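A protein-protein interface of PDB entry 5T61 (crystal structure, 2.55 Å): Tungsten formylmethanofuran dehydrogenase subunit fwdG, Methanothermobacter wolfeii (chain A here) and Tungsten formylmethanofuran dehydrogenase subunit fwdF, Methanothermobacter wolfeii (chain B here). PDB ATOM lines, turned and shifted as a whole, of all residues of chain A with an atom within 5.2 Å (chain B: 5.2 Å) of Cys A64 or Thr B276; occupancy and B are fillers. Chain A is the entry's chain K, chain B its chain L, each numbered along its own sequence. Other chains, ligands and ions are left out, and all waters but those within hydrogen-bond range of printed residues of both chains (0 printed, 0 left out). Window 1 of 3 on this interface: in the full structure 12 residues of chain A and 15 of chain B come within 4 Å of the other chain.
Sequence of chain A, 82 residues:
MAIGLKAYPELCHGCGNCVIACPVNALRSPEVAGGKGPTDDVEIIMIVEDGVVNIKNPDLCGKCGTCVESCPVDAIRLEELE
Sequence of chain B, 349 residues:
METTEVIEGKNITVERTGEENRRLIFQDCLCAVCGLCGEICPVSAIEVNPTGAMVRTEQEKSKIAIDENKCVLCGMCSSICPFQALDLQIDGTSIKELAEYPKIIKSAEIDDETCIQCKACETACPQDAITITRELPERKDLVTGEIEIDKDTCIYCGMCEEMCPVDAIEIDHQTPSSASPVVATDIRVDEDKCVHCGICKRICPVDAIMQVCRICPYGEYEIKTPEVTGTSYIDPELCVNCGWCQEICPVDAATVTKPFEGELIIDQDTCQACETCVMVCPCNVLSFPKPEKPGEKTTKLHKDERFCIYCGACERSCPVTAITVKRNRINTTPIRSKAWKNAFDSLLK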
ATOM      1  N   PRO A  23      14.992  21.520  -3.749  1.00  0.00           N
ATOM      2  CA  PRO A  23      15.721  20.587  -4.623  1.00  0.00           C
ATOM      3  C   PRO A  23      15.407  20.768  -6.095  1.00  0.00           C
ATOM      4  O   PRO A  23      16.292  20.547  -6.931  1.00  0.00           O
ATOM      5  CB  PRO A  23      15.284  19.205  -4.118  1.00  0.00           C
ATOM      6  CG  PRO A  23      14.029  19.433  -3.369  1.00  0.00           C
ATOM      7  CD  PRO A  23      14.010  20.844  -2.884  1.00  0.00           C
ATOM      8  N   GLY A  62       6.658  20.267  -5.872  1.00  0.00           N
ATOM      9  CA  GLY A  62       6.174  18.990  -5.395  1.00  0.00           C
ATOM     10  C   GLY A  62       5.690  18.992  -3.961  1.00  0.00           C
ATOM     11  O   GLY A  62       5.397  17.920  -3.423  1.00  0.00           O
ATOM     12  N   LYS A  63       5.602  20.169  -3.337  1.00  0.00           N
ATOM     13  CA  LYS A  63       5.110  20.336  -1.966  1.00  0.00           C
ATOM     14  C   LYS A  63       5.816  19.393  -0.992  1.00  0.00           C
ATOM     15  O   LYS A  63       5.181  18.707  -0.189  1.00  0.00           O
ATOM     16  CB  LYS A  63       3.591  20.148  -1.881  1.00  0.00           C
ATOM     17  CG  LYS A  63       2.751  21.056  -2.771  1.00  0.00           C
ATOM     18  CD  LYS A  63       2.436  20.396  -4.102  1.00  0.00           C
ATOM     19  CE  LYS A  63       1.608  21.311  -4.984  1.00  0.00           C
ATOM     20  NZ  LYS A  63       1.150  20.626  -6.225  1.00  0.00           N
ATOM     21  N   CYS A  64       7.147  19.365  -1.054  1.00  0.00           N
ATOM     22  CA  CYS A  64       7.871  18.486  -0.141  1.00  0.00           C
ATOM     23  C   CYS A  64       8.011  19.106   1.244  1.00  0.00           C
ATOM     24  O   CYS A  64       8.048  18.376   2.239  1.00  0.00           O
ATOM     25  CB  CYS A  64       9.251  18.124  -0.698  1.00  0.00           C
ATOM     26  SG  CYS A  64      10.547  19.326  -0.376  1.00  0.00           S
ATOM     27  N   GLY A  65       8.098  20.434   1.328  1.00  0.00           N
ATOM     28  CA  GLY A  65       8.144  21.133   2.595  1.00  0.00           C
ATOM     29  C   GLY A  65       9.501  21.660   3.003  1.00  0.00           C
ATOM     30  O   GLY A  65       9.614  22.267   4.075  1.00  0.00           O
ATOM     31  N   THR A  66      10.530  21.465   2.177  1.00  0.00           N
ATOM     32  CA  THR A  66      11.881  21.859   2.563  1.00  0.00           C
ATOM     33  C   THR A  66      11.988  23.371   2.708  1.00  0.00           C
ATOM     34  O   THR A  66      12.564  23.874   3.680  1.00  0.00           O
ATOM     35  CB  THR A  66      12.888  21.336   1.540  1.00  0.00           C
ATOM     36  OG1 THR A  66      12.693  19.927   1.361  1.00  0.00           O
ATOM     37  CG2 THR A  66      14.313  21.596   2.005  1.00  0.00           C
ATOM     38  N   LEU A  78       3.010  26.107   2.691  1.00  0.00           N
ATOM     39  CA  LEU A  78       2.167  25.136   2.008  1.00  0.00           C
ATOM     40  C   LEU A  78       0.804  25.165   2.689  1.00  0.00           C
ATOM     41  O   LEU A  78       0.683  24.779   3.857  1.00  0.00           O
ATOM     42  CB  LEU A  78       2.781  23.740   2.065  1.00  0.00           C
ATOM     43  CG  LEU A  78       4.095  23.597   1.305  1.00  0.00           C
ATOM     44  CD1 LEU A  78       4.738  22.262   1.623  1.00  0.00           C
ATOM     45  CD2 LEU A  78       3.866  23.760  -0.190  1.00  0.00           C
ATOM     46  N   GLY B  52       5.271  14.733   1.466  1.00  0.00           N
ATOM     47  CA  GLY B  52       6.228  15.588   2.153  1.00  0.00           C
ATOM     48  C   GLY B  52       5.567  16.641   3.022  1.00  0.00           C
ATOM     49  O   GLY B  52       5.924  16.812   4.190  1.00  0.00           O
ATOM     50  N   ALA B  53       4.604  17.372   2.454  1.00  0.00           N
ATOM     51  CA  ALA B  53       3.932  18.440   3.194  1.00  0.00           C
ATOM     52  C   ALA B  53       3.270  17.922   4.467  1.00  0.00           C
ATOM     53  O   ALA B  53       3.334  18.575   5.516  1.00  0.00           O
ATOM     54  CB  ALA B  53       2.900  19.124   2.298  1.00  0.00           C
ATOM     55  N   ARG B  56       6.347  17.020   6.965  1.00  0.00           N
ATOM     56  CA  ARG B  56       7.332  18.023   7.354  1.00  0.00           C
ATOM     57  C   ARG B  56       6.729  19.330   7.851  1.00  0.00           C
ATOM     58  O   ARG B  56       7.443  20.118   8.478  1.00  0.00           O
ATOM     59  CB  ARG B  56       8.265  18.342   6.176  1.00  0.00           C
ATOM     60  CG  ARG B  56       9.160  17.200   5.731  1.00  0.00           C
ATOM     61  CD  ARG B  56      10.183  17.706   4.723  1.00  0.00           C
ATOM     62  NE  ARG B  56      11.202  18.539   5.358  1.00  0.00           N
ATOM     63  CZ  ARG B  56      12.413  18.761   4.855  1.00  0.00           C
ATOM     64  NH1 ARG B  56      13.272  19.531   5.512  1.00  0.00           N
ATOM     65  NH2 ARG B  56      12.758  18.241   3.688  1.00  0.00           N
ATOM     66  N   CYS B 274      17.449  17.084  -0.144  1.00  0.00           N
ATOM     67  CA  CYS B 274      16.567  17.938   0.646  1.00  0.00           C
ATOM     68  C   CYS B 274      16.109  17.264   1.937  1.00  0.00           C
ATOM     69  O   CYS B 274      15.492  17.935   2.769  1.00  0.00           O
ATOM     70  CB  CYS B 274      15.360  18.407  -0.176  1.00  0.00           C
ATOM     71  SG  CYS B 274      13.911  17.342  -0.216  1.00  0.00           S
ATOM     72  N   GLU B 275      16.347  15.959   2.086  1.00  0.00           N
ATOM     73  CA  GLU B 275      16.097  15.112   3.262  1.00  0.00           C
ATOM     74  C   GLU B 275      14.631  14.701   3.401  1.00  0.00           C
ATOM     75  O   GLU B 275      14.290  14.026   4.383  1.00  0.00           O
ATOM     76  CB  GLU B 275      16.557  15.760   4.581  1.00  0.00           C
ATOM     77  CG  GLU B 275      16.863  14.765   5.708  1.00  0.00           C
ATOM     78  CD  GLU B 275      17.591  15.395   6.883  1.00  0.00           C
ATOM     79  OE1 GLU B 275      17.486  14.850   8.002  1.00  0.00           O
ATOM     80  OE2 GLU B 275      18.253  16.438   6.697  1.00  0.00           O
ATOM     81  N   THR B 276      13.761  15.049   2.451  1.00  0.00           N
ATOM     82  CA  THR B 276      12.341  14.741   2.597  1.00  0.00           C
ATOM     83  C   THR B 276      12.100  13.240   2.731  1.00  0.00           C
ATOM     84  O   THR B 276      11.455  12.786   3.684  1.00  0.00           O
ATOM     85  CB  THR B 276      11.555  15.304   1.414  1.00  0.00           C
ATOM     86  OG1 THR B 276      11.717  16.727   1.365  1.00  0.00           O
ATOM     87  CG2 THR B 276      10.085  14.978   1.563  1.00  0.00           C
ATOM     88  N   CYS B 277      12.599  12.450   1.774  1.00  0.00           N
ATOM     89  CA  CYS B 277      12.343  11.011   1.808  1.00  0.00           C
ATOM     90  C   CYS B 277      12.912  10.375   3.067  1.00  0.00           C
ATOM     91  O   CYS B 277      12.331   9.422   3.600  1.00  0.00           O
ATOM     92  CB  CYS B 277      12.940  10.326   0.583  1.00  0.00           C
ATOM     93  SG  CYS B 277      14.700   9.999   0.775  1.00  0.00           S
ATOM     94  N   VAL B 278      14.056  10.875   3.539  1.00  0.00           N
ATOM     95  CA  VAL B 278      14.653  10.356   4.765  1.00  0.00           C
ATOM     96  C   VAL B 278      13.697  10.539   5.934  1.00  0.00           C
ATOM     97  O   VAL B 278      13.465   9.615   6.723  1.00  0.00           O
ATOM     98  CB  VAL B 278      16.007  11.039   5.031  1.00  0.00           C
ATOM     99  CG1 VAL B 278      16.526  10.667   6.409  1.00  0.00           C
ATOM    100  CG2 VAL B 278      17.006  10.637   3.960  1.00  0.00           C
ATOM    101  N   MET B 279      13.099  11.729   6.037  1.00  0.00           N
ATOM    102  CA  MET B 279      12.147  12.019   7.103  1.00  0.00           C
ATOM    103  C   MET B 279      10.828  11.287   6.883  1.00  0.00           C
ATOM    104  O   MET B 279      10.157  10.907   7.850  1.00  0.00           O
ATOM    105  CB  MET B 279      11.907  13.530   7.159  1.00  0.00           C
ATOM    106  CG  MET B 279      13.164  14.367   7.376  1.00  0.00           C
ATOM    107  SD  MET B 279      12.918  16.152   7.156  1.00  0.00           S
ATOM    108  CE  MET B 279      12.174  16.638   8.702  1.00  0.00           C
ATOM    109  N   VAL B 280      10.457  11.072   5.619  1.00  0.00           N
ATOM    110  CA  VAL B 280       9.193  10.423   5.289  1.00  0.00           C
ATOM    111  C   VAL B 280       9.245   8.927   5.590  1.00  0.00           C
ATOM    112  O   VAL B 280       8.262   8.343   6.065  1.00  0.00           O
ATOM    113  CB  VAL B 280       8.830  10.703   3.819  1.00  0.00           C
ATOM    114  CG1 VAL B 280       7.944   9.608   3.259  1.00  0.00           C
ATOM    115  CG2 VAL B 280       8.140  12.056   3.698  1.00  0.00           C
ATOM    116  N   CYS B 281      10.384   8.283   5.310  1.00  0.00           N
ATOM    117  CA  CYS B 281      10.509   6.831   5.405  1.00  0.00           C
ATOM    118  C   CYS B 281      10.052   6.311   6.759  1.00  0.00           C
ATOM    119  O   CYS B 281      10.698   6.570   7.782  1.00  0.00           O
ATOM    120  CB  CYS B 281      11.950   6.395   5.158  1.00  0.00           C
ATOM    121  SG  CYS B 281      12.255   4.683   5.632  1.00  0.00           S
ATOM    122  N   SER B 317       7.088  11.369  -2.158  1.00  0.00           N
ATOM    123  CA  SER B 317       7.468  12.630  -1.532  1.00  0.00           C
ATOM    124  C   SER B 317       8.533  13.393  -2.313  1.00  0.00           C
ATOM    125  O   SER B 317       8.655  14.610  -2.133  1.00  0.00           O
ATOM    126  CB  SER B 317       7.969  12.386  -0.104  1.00  0.00           C
ATOM    127  OG  SER B 317       9.245  11.765  -0.097  1.00  0.00           O
ATOM    128  N   PRO B 319      10.316  15.584  -4.843  1.00  0.00           N
ATOM    129  CA  PRO B 319       9.877  16.526  -5.880  1.00  0.00           C
ATOM    130  C   PRO B 319      10.676  16.458  -7.177  1.00  0.00           C
ATOM    131  O   PRO B 319      10.282  17.115  -8.149  1.00  0.00           O
ATOM    132  CB  PRO B 319      10.048  17.888  -5.198  1.00  0.00           C
ATOM    133  CG  PRO B 319      11.136  17.677  -4.213  1.00  0.00           C
ATOM    134  CD  PRO B 319      11.053  16.250  -3.754  1.00  0.00           C
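Hydrophobic or aromatic side chains of chain B that line the printed part of chain A: Ala B53 and Pro B319.
Among the printed residues, 14 pairs touch across the chains.
Among the printed residues, no Asp or Glu carboxylate lies within 4 Å of a Lys or Arg side-chain nitrogen of the other chain.
Pro A23 touches Cys B274 (CG to CB, 3.6 Å).
Pro B319 touches Pro A23 (CG to CG, 3.5 Å).
O of Lys A63 touches C of Gly B52, 3.8 Å away.
O of Cys A64 touches N of Ala B53, 3.6 Å away.
Cys A64 touches Arg B56 (O to CD, 3.3 Å).
Cys A64 touches Cys B274 (SG to SG, 3.9 Å).
Ser B317 touches Cys A64.
CD1 of Leu A78 touches CB of Ala B53 (3.7 Å).
The backbone NH (N) of Ala B53 is in hydrogen-bond range of the backbone carbonyl oxygen (O) of Lys A63 (3.0 Å).
OG1 of Thr B276 sits close to SG of Cys A64, at 3.3 Å.
OG1 of Thr A66 sits at hydrogen-bond distance from NH2 of Arg B56, 2.9 Å away.
SG of Cys B274 lies close to OG1 of Thr A66.
The side-chain hydroxyl (OG1) of Thr B276 is in hydrogen-bond range of the side-chain hydroxyl (OG1) of Thr A66 (3.3 Å).
O of Cys A64 sits close to O of Gly B52, at 3.3 Å.
Printed residues of chain B within 4 Å of Cys A64: Gly B52, Ala B53, Arg B56, Cys B274, Thr B276 and Ser B317.
Of chain A, only Cys A64 (3.3 Å) and Thr A66 (3.3 Å) come within 4 Å of Thr B276.
Of the printed residues of chain B, Leu A78 touches Ala B53 (3.7 Å).
Of the printed residues of chain A, Ser B317 touches Cys A64 (3.8 Å).
The nearest printed residue of chain B that does not touch Cys A64 is Pro B319 (4.01 Å).
The nearest printed residue of chain A that does not touch Gly B52 is Gly A65 (4.9 Å).
The side-chain sulfur (SG) of Cys A64 lies close to the side-chain hydroxyl (OG1) of Thr A66, at 2.8 Å.
NH2 of Arg B56 sits at hydrogen-bond distance from O of Cys B274 (2.9 Å).
NH2 of Arg B56 sits at hydrogen-bond distance from OG1 of Thr B276, at 3.0 Å.
The side-chain sulfur (SD) of Met B279 is in hydrogen-bond range of the guanidinium group (NE) of Arg B56, at 3.4 Å.
The side-chain sulfur of Cys B274 lies close to the side-chain hydroxyl of Thr B276.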
